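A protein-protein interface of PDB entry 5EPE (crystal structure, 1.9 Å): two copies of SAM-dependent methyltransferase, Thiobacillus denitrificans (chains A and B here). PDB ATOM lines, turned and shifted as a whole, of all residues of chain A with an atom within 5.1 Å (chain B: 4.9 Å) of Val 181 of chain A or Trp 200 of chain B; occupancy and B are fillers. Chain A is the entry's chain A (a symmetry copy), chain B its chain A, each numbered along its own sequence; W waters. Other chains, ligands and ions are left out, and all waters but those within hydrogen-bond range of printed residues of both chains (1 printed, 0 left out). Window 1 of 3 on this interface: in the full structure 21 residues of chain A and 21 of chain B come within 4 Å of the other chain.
The side-chain hydroxyl of Thr 202 of chain B lies within hydrogen-bond range of the backbone carbonyl oxygen of Ala 198 of chain B, 3.1 Å away.
The backbone carbonyl oxygen (O) of Ala 244 of chain A sits at hydrogen-bond distance from the backbone NH (N) of Val 182 of chain A (2.8 Å).
The backbone NH of Ala 244 of chain A lies within hydrogen-bond range of the backbone carbonyl oxygen of Glu 183 of chain A (2.9 Å).
The indole nitrogen (NE1) of Trp 200 of chain B is in hydrogen-bond range of the backbone carbonyl oxygen (O) of Glu 196 of chain B (3.3 Å).
Leu 171 of chain A touches Pro 227 of chain B (CD1 to O, 3.7 Å).
CD2 of Leu 223 of chain B touches OD2 of Asp 180 of chain A, 3.6 Å away.
O of Val 181 of chain A touches CE3 of Trp 200 of chain B (3.5 Å).
Val 182 of chain A touches Trp 200 of chain B.
CG1 of Val 182 of chain A touches CB of Arg 204 of chain B, 3.97 Å away.
OE2 of Glu 183 of chain A touches CB of Ala 197 of chain B (3.4 Å).
Ala 197 of chain B touches Met 184 of chain A.
Tyr 230 of chain B touches Met 184 of chain A.
Water W1 bridges the backbone carbonyl oxygen of Leu 223 of chain B and the backbone carbonyl oxygen of Val 181 of chain A.
The backbone carbonyl oxygen (O) of Val 182 of chain A lies close to the backbone carbonyl oxygen (O) of Ala 197 of chain B, 3.3 Å away.
OD2 of Asp 180 of chain A is in salt-bridge range of NH1 of Arg 204 of chain B (2.8 Å).
The backbone carbonyl oxygen (O) of Val 182 of chain A sits at hydrogen-bond distance from the backbone NH (N) of Leu 201 of chain B, 3.0 Å away.
The backbone NH (N) of Ala 198 of chain B lies close to the side-chain carboxylate (OE1) of Glu 183 of chain A.
Hydrophobic or aromatic side chains of chain B within 4 Å of the printed part of chain A: Ala 197, Ala 198, Trp 200, Leu 201, Leu 223 and Tyr 230.
Of the 11 printed residues of chain A, 6 touch a printed residue of chain B.
Printed residues of chain A that touch a printed residue of chain B: Leu 171, Asp 180, Val 181, Val 182, Glu 183 and Met 184.
Hydrophobic or aromatic side chains of chain A within 4 Å of the printed part of chain B: Leu 171, Val 181, Val 182 and Met 184.
Among the printed residues, Asp or Glu carboxylates within 4 Å of a Lys or Arg side-chain nitrogen of the other chain: Asp 180 of chain A with Arg 204 of chain B (2.8 Å).
Of the printed residues of chain B, Leu 171 of chain A touches Pro 227.
Tyr 179 of chain A touches none of the printed residues of chain B.
Of chain B, only Trp 200 comes within 4 Å of Val 181 of chain A.
Trp 200 of chain B touches just these residues of chain A: Val 181 (3.5 Å) and Val 182 (3.7 Å).
Of the printed residues of chain A, Leu 201 of chain B touches Val 182 (3.0 Å).
Printed residues of chain A within 4 Å of Pro 227 of chain B: Leu 171 (3.7 Å).
The nearest residue of chain B that does not touch Val 181 of chain A is Pro 227 of chain B (4.03 Å).
The nearest printed residue of chain A that does not touch Trp 200 of chain B is Met 184 of chain A (4.1 Å).
The nearest printed residue of chain A that does not touch Ala 197 of chain B is Val 181 of chain A (6.0 Å).
No position is printed for both chains.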
ATOM      1  N   LEU A 171      -6.866 -27.659  26.809  1.00  0.00           N
ATOM      2  CA  LEU A 171      -8.133 -27.046  27.204  1.00  0.00           C
ATOM      3  C   LEU A 171      -8.549 -27.403  28.616  1.00  0.00           C
ATOM      4  O   LEU A 171      -8.957 -26.519  29.386  1.00  0.00           O
ATOM      5  CB  LEU A 171      -9.237 -27.380  26.207  1.00  0.00           C
ATOM      6  CG  LEU A 171      -9.059 -26.777  24.812  1.00  0.00           C
ATOM      7  CD1 LEU A 171     -10.003 -27.474  23.853  1.00  0.00           C
ATOM      8  CD2 LEU A 171      -9.325 -25.287  24.899  1.00  0.00           C
ATOM      9  N   PHE A 174      -6.776 -25.261  31.368  1.00  0.00           N
ATOM     10  CA  PHE A 174      -7.431 -23.980  31.711  1.00  0.00           C
ATOM     11  C   PHE A 174      -8.632 -24.167  32.644  1.00  0.00           C
ATOM     12  O   PHE A 174      -8.788 -23.407  33.625  1.00  0.00           O
ATOM     13  CB  PHE A 174      -7.880 -23.250  30.458  1.00  0.00           C
ATOM     14  CG  PHE A 174      -6.758 -22.819  29.553  1.00  0.00           C
ATOM     15  CD1 PHE A 174      -5.825 -21.912  29.988  1.00  0.00           C
ATOM     16  CD2 PHE A 174      -6.670 -23.293  28.256  1.00  0.00           C
ATOM     17  CE1 PHE A 174      -4.821 -21.460  29.136  1.00  0.00           C
ATOM     18  CE2 PHE A 174      -5.688 -22.813  27.380  1.00  0.00           C
ATOM     19  CZ  PHE A 174      -4.759 -21.914  27.831  1.00  0.00           C
ATOM     20  N   TYR A 179     -10.869 -21.533  35.039  1.00  0.00           N
ATOM     21  CA  TYR A 179     -11.366 -20.653  33.955  1.00  0.00           C
ATOM     22  C   TYR A 179     -12.237 -21.404  33.002  1.00  0.00           C
ATOM     23  O   TYR A 179     -11.935 -22.550  32.671  1.00  0.00           O
ATOM     24  CB  TYR A 179     -10.170 -20.043  33.176  1.00  0.00           C
ATOM     25  CG  TYR A 179      -9.456 -19.099  34.077  1.00  0.00           C
ATOM     26  CD1 TYR A 179      -8.547 -19.560  35.043  1.00  0.00           C
ATOM     27  CD2 TYR A 179      -9.769 -17.755  34.058  1.00  0.00           C
ATOM     28  CE1 TYR A 179      -7.950 -18.695  35.937  1.00  0.00           C
ATOM     29  CE2 TYR A 179      -9.146 -16.884  34.927  1.00  0.00           C
ATOM     30  CZ  TYR A 179      -8.259 -17.354  35.865  1.00  0.00           C
ATOM     31  OH  TYR A 179      -7.677 -16.423  36.699  1.00  0.00           O
ATOM     32  N   ASP A 180     -13.288 -20.756  32.511  1.00  0.00           N
ATOM     33  CA  ASP A 180     -13.985 -21.249  31.337  1.00  0.00           C
ATOM     34  C   ASP A 180     -13.205 -20.772  30.099  1.00  0.00           C
ATOM     35  O   ASP A 180     -12.842 -19.582  30.021  1.00  0.00           O
ATOM     36  CB  ASP A 180     -15.389 -20.665  31.246  1.00  0.00           C
ATOM     37  CG  ASP A 180     -16.351 -21.225  32.324  1.00  0.00           C
ATOM     38  OD1 ASP A 180     -16.268 -22.432  32.700  1.00  0.00           O
ATOM     39  OD2 ASP A 180     -17.264 -20.459  32.696  1.00  0.00           O
ATOM     40  N   VAL A 181     -13.014 -21.671  29.137  1.00  0.00           N
ATOM     41  CA  VAL A 181     -12.589 -21.289  27.827  1.00  0.00           C
ATOM     42  C   VAL A 181     -13.824 -20.838  27.080  1.00  0.00           C
ATOM     43  O   VAL A 181     -14.746 -21.658  26.814  1.00  0.00           O
ATOM     44  CB  VAL A 181     -11.874 -22.436  27.053  1.00  0.00           C
ATOM     45  CG1 VAL A 181     -11.547 -22.023  25.624  1.00  0.00           C
ATOM     46  CG2 VAL A 181     -10.621 -22.891  27.817  1.00  0.00           C
ATOM     47  N   VAL A 182     -13.860 -19.567  26.707  1.00  0.00           N
ATOM     48  CA  VAL A 182     -15.046 -19.015  26.053  1.00  0.00           C
ATOM     49  C   VAL A 182     -14.925 -18.769  24.570  1.00  0.00           C
ATOM     50  O   VAL A 182     -15.918 -18.414  23.938  1.00  0.00           O
ATOM     51  CB  VAL A 182     -15.534 -17.729  26.760  1.00  0.00           C
ATOM     52  CG1 VAL A 182     -15.950 -18.067  28.176  1.00  0.00           C
ATOM     53  CG2 VAL A 182     -14.475 -16.641  26.730  1.00  0.00           C
ATOM     54  N   GLU A 183     -13.702 -18.849  24.041  1.00  0.00           N
ATOM     55  CA  GLU A 183     -13.462 -18.737  22.617  1.00  0.00           C
ATOM     56  C   GLU A 183     -12.058 -19.218  22.331  1.00  0.00           C
ATOM     57  O   GLU A 183     -11.212 -19.265  23.217  1.00  0.00           O
ATOM     58  CB  GLU A 183     -13.695 -17.315  22.092  1.00  0.00           C
ATOM     59  CG  GLU A 183     -14.993 -17.153  21.257  1.00  0.00           C
ATOM     60  CD  GLU A 183     -14.926 -17.746  19.840  1.00  0.00           C
ATOM     61  OE1 GLU A 183     -15.847 -17.517  19.000  1.00  0.00           O
ATOM     62  OE2 GLU A 183     -13.901 -18.414  19.517  1.00  0.00           O
ATOM     63  N   MET A 184     -11.814 -19.521  21.059  1.00  0.00           N
ATOM     64  CA  MET A 184     -10.456 -19.847  20.624  1.00  0.00           C
ATOM     65  C   MET A 184     -10.323 -19.740  19.143  1.00  0.00           C
ATOM     66  O   MET A 184     -11.278 -20.054  18.392  1.00  0.00           O
ATOM     67  CB  MET A 184      -9.908 -21.223  21.096  1.00  0.00           C
ATOM     68  CG  MET A 184     -10.720 -22.313  20.504  1.00  0.00           C
ATOM     69  SD  MET A 184     -10.182 -24.147  21.125  1.00  0.00           S
ATOM     70  CE  MET A 184     -11.075 -25.158  19.721  1.00  0.00           C
ATOM     71  N   PHE A 243      -6.487 -18.506  23.175  1.00  0.00           N
ATOM     72  CA  PHE A 243      -7.550 -18.984  24.020  1.00  0.00           C
ATOM     73  C   PHE A 243      -8.076 -17.837  24.875  1.00  0.00           C
ATOM     74  O   PHE A 243      -7.305 -17.130  25.537  1.00  0.00           O
ATOM     75  CB  PHE A 243      -7.008 -20.114  24.880  1.00  0.00           C
ATOM     76  CG  PHE A 243      -6.435 -21.239  24.074  1.00  0.00           C
ATOM     77  CD1 PHE A 243      -5.120 -21.216  23.686  1.00  0.00           C
ATOM     78  CD2 PHE A 243      -7.232 -22.327  23.703  1.00  0.00           C
ATOM     79  CE1 PHE A 243      -4.599 -22.256  22.913  1.00  0.00           C
ATOM     80  CE2 PHE A 243      -6.691 -23.405  23.013  1.00  0.00           C
ATOM     81  CZ  PHE A 243      -5.388 -23.336  22.577  1.00  0.00           C
ATOM     82  N   ALA A 244      -9.392 -17.665  24.852  1.00  0.00           N
ATOM     83  CA  ALA A 244     -10.081 -16.638  25.605  1.00  0.00           C
ATOM     84  C   ALA A 244     -10.682 -17.247  26.840  1.00  0.00           C
ATOM     85  O   ALA A 244     -11.381 -18.258  26.767  1.00  0.00           O
ATOM     86  CB  ALA A 244     -11.189 -15.991  24.732  1.00  0.00           C
ATOM     87  N   LEU A 245     -10.391 -16.637  27.983  1.00  0.00           N
ATOM     88  CA  LEU A 245     -10.668 -17.198  29.321  1.00  0.00           C
ATOM     89  C   LEU A 245     -11.515 -16.222  30.141  1.00  0.00           C
ATOM     90  O   LEU A 245     -11.275 -14.998  30.119  1.00  0.00           O
ATOM     91  CB  LEU A 245      -9.383 -17.461  30.081  1.00  0.00           C
ATOM     92  CG  LEU A 245      -8.297 -18.236  29.312  1.00  0.00           C
ATOM     93  CD1 LEU A 245      -7.094 -18.392  30.211  1.00  0.00           C
ATOM     94  CD2 LEU A 245      -8.806 -19.614  28.920  1.00  0.00           C
ATOM     95  N   GLU B 196     -18.527 -23.875  16.872  1.00  0.00           N
ATOM     96  CA  GLU B 196     -18.601 -24.414  18.208  1.00  0.00           C
ATOM     97  C   GLU B 196     -18.145 -23.435  19.265  1.00  0.00           C
ATOM     98  O   GLU B 196     -18.853 -23.216  20.259  1.00  0.00           O
ATOM     99  CB  GLU B 196     -17.827 -25.733  18.318  1.00  0.00           C
ATOM    100  CG  GLU B 196     -18.467 -26.839  17.473  1.00  0.00           C
ATOM    101  CD  GLU B 196     -19.832 -27.340  17.971  1.00  0.00           C
ATOM    102  OE1 GLU B 196     -20.362 -26.879  19.021  1.00  0.00           O
ATOM    103  OE2 GLU B 196     -20.378 -28.230  17.274  1.00  0.00           O
ATOM    104  N   ALA B 197     -16.982 -22.825  19.068  1.00  0.00           N
ATOM    105  CA  ALA B 197     -16.426 -21.946  20.091  1.00  0.00           C
ATOM    106  C   ALA B 197     -17.221 -20.718  20.379  1.00  0.00           C
ATOM    107  O   ALA B 197     -17.262 -20.226  21.538  1.00  0.00           O
ATOM    108  CB  ALA B 197     -14.982 -21.605  19.805  1.00  0.00           C
ATOM    109  N   ALA B 198     -17.881 -20.204  19.358  1.00  0.00           N
ATOM    110  CA  ALA B 198     -18.735 -19.035  19.555  1.00  0.00           C
ATOM    111  C   ALA B 198     -19.868 -19.331  20.491  1.00  0.00           C
ATOM    112  O   ALA B 198     -20.376 -18.414  21.133  1.00  0.00           O
ATOM    113  CB  ALA B 198     -19.296 -18.531  18.203  1.00  0.00           C
ATOM    114  N   LYS B 199     -20.319 -20.591  20.547  1.00  0.00           N
ATOM    115  CA  LYS B 199     -21.382 -20.952  21.485  1.00  0.00           C
ATOM    116  C   LYS B 199     -20.941 -20.772  22.922  1.00  0.00           C
ATOM    117  O   LYS B 199     -21.747 -20.433  23.770  1.00  0.00           O
ATOM    118  CB  LYS B 199     -21.805 -22.399  21.304  1.00  0.00           C
ATOM    119  CG  LYS B 199     -22.361 -22.746  19.932  1.00  0.00           C
ATOM    120  CD  LYS B 199     -22.632 -24.248  19.867  1.00  0.00           C
ATOM    121  CE  LYS B 199     -23.085 -24.671  18.486  1.00  0.00           C
ATOM    122  NZ  LYS B 199     -23.278 -26.149  18.552  1.00  0.00           N
ATOM    123  N   TRP B 200     -19.642 -20.955  23.197  1.00  0.00           N
ATOM    124  CA  TRP B 200     -19.182 -20.914  24.572  1.00  0.00           C
ATOM    125  C   TRP B 200     -19.268 -19.493  25.135  1.00  0.00           C
ATOM    126  O   TRP B 200     -19.730 -19.309  26.257  1.00  0.00           O
ATOM    127  CB  TRP B 200     -17.754 -21.485  24.710  1.00  0.00           C
ATOM    128  CG  TRP B 200     -17.556 -22.779  23.991  1.00  0.00           C
ATOM    129  CD1 TRP B 200     -18.475 -23.748  23.733  1.00  0.00           C
ATOM    130  CD2 TRP B 200     -16.321 -23.241  23.465  1.00  0.00           C
ATOM    131  NE1 TRP B 200     -17.905 -24.769  23.009  1.00  0.00           N
ATOM    132  CE2 TRP B 200     -16.575 -24.479  22.829  1.00  0.00           C
ATOM    133  CE3 TRP B 200     -15.026 -22.719  23.458  1.00  0.00           C
ATOM    134  CZ2 TRP B 200     -15.595 -25.190  22.193  1.00  0.00           C
ATOM    135  CZ3 TRP B 200     -14.028 -23.447  22.837  1.00  0.00           C
ATOM    136  CH2 TRP B 200     -14.329 -24.673  22.216  1.00  0.00           C
ATOM    137  N   LEU B 201     -18.870 -18.498  24.352  1.00  0.00           N
ATOM    138  CA  LEU B 201     -18.942 -17.109  24.820  1.00  0.00           C
ATOM    139  C   LEU B 201     -20.408 -16.699  25.016  1.00  0.00           C
ATOM    140  O   LEU B 201     -20.766 -16.078  26.000  1.00  0.00           O
ATOM    141  CB  LEU B 201     -18.229 -16.191  23.816  1.00  0.00           C
ATOM    142  CG  LEU B 201     -18.210 -14.703  24.193  1.00  0.00           C
ATOM    143  CD1 LEU B 201     -17.568 -14.511  25.542  1.00  0.00           C
ATOM    144  CD2 LEU B 201     -17.532 -13.844  23.125  1.00  0.00           C
ATOM    145  N   THR B 202     -21.249 -17.067  24.046  1.00  0.00           N
ATOM    146  CA  THR B 202     -22.657 -16.799  24.136  1.00  0.00           C
ATOM    147  C   THR B 202     -23.270 -17.398  25.437  1.00  0.00           C
ATOM    148  O   THR B 202     -24.007 -16.729  26.150  1.00  0.00           O
ATOM    149  CB  THR B 202     -23.406 -17.291  22.893  1.00  0.00           C
ATOM    150  OG1 THR B 202     -22.857 -16.624  21.743  1.00  0.00           O
ATOM    151  CG2 THR B 202     -24.967 -16.957  22.993  1.00  0.00           C
ATOM    152  N   MET B 203     -22.988 -18.663  25.680  1.00  0.00           N
ATOM    153  CA  MET B 203     -23.475 -19.350  26.856  1.00  0.00           C
ATOM    154  C   MET B 203     -23.011 -18.733  28.134  1.00  0.00           C
ATOM    155  O   MET B 203     -23.791 -18.603  29.076  1.00  0.00           O
ATOM    156  CB  MET B 203     -23.104 -20.821  26.847  1.00  0.00           C
ATOM    157  CG  MET B 203     -23.971 -21.645  25.926  1.00  0.00           C
ATOM    158  SD  MET B 203     -23.358 -23.572  26.080  1.00  0.00           S
ATOM    159  CE  MET B 203     -21.922 -23.349  24.937  1.00  0.00           C
ATOM    160  N   ARG B 204     -21.743 -18.353  28.211  1.00  0.00           N
ATOM    161  CA  ARG B 204     -21.230 -17.766  29.440  1.00  0.00           C
ATOM    162  C   ARG B 204     -21.862 -16.425  29.755  1.00  0.00           C
ATOM    163  O   ARG B 204     -22.237 -16.165  30.930  1.00  0.00           O
ATOM    164  CB  ARG B 204     -19.699 -17.576  29.393  1.00  0.00           C
ATOM    165  CG  ARG B 204     -19.088 -16.926  30.646  1.00  0.00           C
ATOM    166  CD  ARG B 204     -19.419 -17.722  31.926  1.00  0.00           C
ATOM    167  NE  ARG B 204     -19.069 -16.939  33.080  1.00  0.00           N
ATOM    168  CZ  ARG B 204     -17.905 -16.961  33.727  1.00  0.00           C
ATOM    169  NH1 ARG B 204     -16.918 -17.803  33.446  1.00  0.00           N
ATOM    170  NH2 ARG B 204     -17.759 -16.136  34.730  1.00  0.00           N
ATOM    171  N   LEU B 223     -21.234 -25.811  29.237  1.00  0.00           N
ATOM    172  CA  LEU B 223     -20.109 -24.917  29.076  1.00  0.00           C
ATOM    173  C   LEU B 223     -18.819 -25.529  29.620  1.00  0.00           C
ATOM    174  O   LEU B 223     -17.773 -25.422  29.007  1.00  0.00           O
ATOM    175  CB  LEU B 223     -20.401 -23.596  29.799  1.00  0.00           C
ATOM    176  CG  LEU B 223     -19.405 -22.489  29.582  1.00  0.00           C
ATOM    177  CD1 LEU B 223     -19.141 -22.178  28.092  1.00  0.00           C
ATOM    178  CD2 LEU B 223     -19.884 -21.277  30.377  1.00  0.00           C
ATOM    179  N   GLU B 226     -18.027 -28.770  27.105  1.00  0.00           N
ATOM    180  CA  GLU B 226     -17.978 -28.701  25.667  1.00  0.00           C
ATOM    181  C   GLU B 226     -16.596 -28.584  24.999  1.00  0.00           C
ATOM    182  O   GLU B 226     -16.440 -29.207  23.972  1.00  0.00           O
ATOM    183  CB  GLU B 226     -18.937 -27.637  25.107  1.00  0.00           C
ATOM    184  CG  GLU B 226     -20.342 -28.191  24.912  1.00  0.00           C
ATOM    185  CD  GLU B 226     -20.386 -29.242  23.807  1.00  0.00           C
ATOM    186  OE1 GLU B 226     -19.878 -29.000  22.660  1.00  0.00           O
ATOM    187  OE2 GLU B 226     -20.903 -30.345  24.098  1.00  0.00           O
ATOM    188  N   PRO B 227     -15.693 -27.696  25.487  1.00  0.00           N
ATOM    189  CA  PRO B 227     -14.453 -27.502  24.739  1.00  0.00           C
ATOM    190  C   PRO B 227     -13.715 -28.845  24.600  1.00  0.00           C
ATOM    191  O   PRO B 227     -13.259 -29.167  23.530  1.00  0.00           O
ATOM    192  CB  PRO B 227     -13.685 -26.478  25.576  1.00  0.00           C
ATOM    193  CG  PRO B 227     -14.802 -25.634  26.188  1.00  0.00           C
ATOM    194  CD  PRO B 227     -15.859 -26.639  26.507  1.00  0.00           C
ATOM    195  N   TYR B 230     -15.666 -31.333  22.303  1.00  0.00           N
ATOM    196  CA  TYR B 230     -15.477 -30.874  20.926  1.00  0.00           C
ATOM    197  C   TYR B 230     -14.062 -31.239  20.404  1.00  0.00           C
ATOM    198  O   TYR B 230     -13.918 -31.795  19.327  1.00  0.00           O
ATOM    199  CB  TYR B 230     -15.744 -29.341  20.830  1.00  0.00           C
ATOM    200  CG  TYR B 230     -15.232 -28.767  19.575  1.00  0.00           C
ATOM    201  CD1 TYR B 230     -15.850 -29.066  18.370  1.00  0.00           C
ATOM    202  CD2 TYR B 230     -14.094 -27.961  19.565  1.00  0.00           C
ATOM    203  CE1 TYR B 230     -15.342 -28.604  17.185  1.00  0.00           C
ATOM    204  CE2 TYR B 230     -13.596 -27.453  18.386  1.00  0.00           C
ATOM    205  CZ  TYR B 230     -14.236 -27.751  17.182  1.00  0.00           C
ATOM    206  OH  TYR B 230     -13.751 -27.307  15.966  1.00  0.00           O
HETATM  207  O   HOH W   1     -15.826 -23.449  28.859  1.00  0.00           O
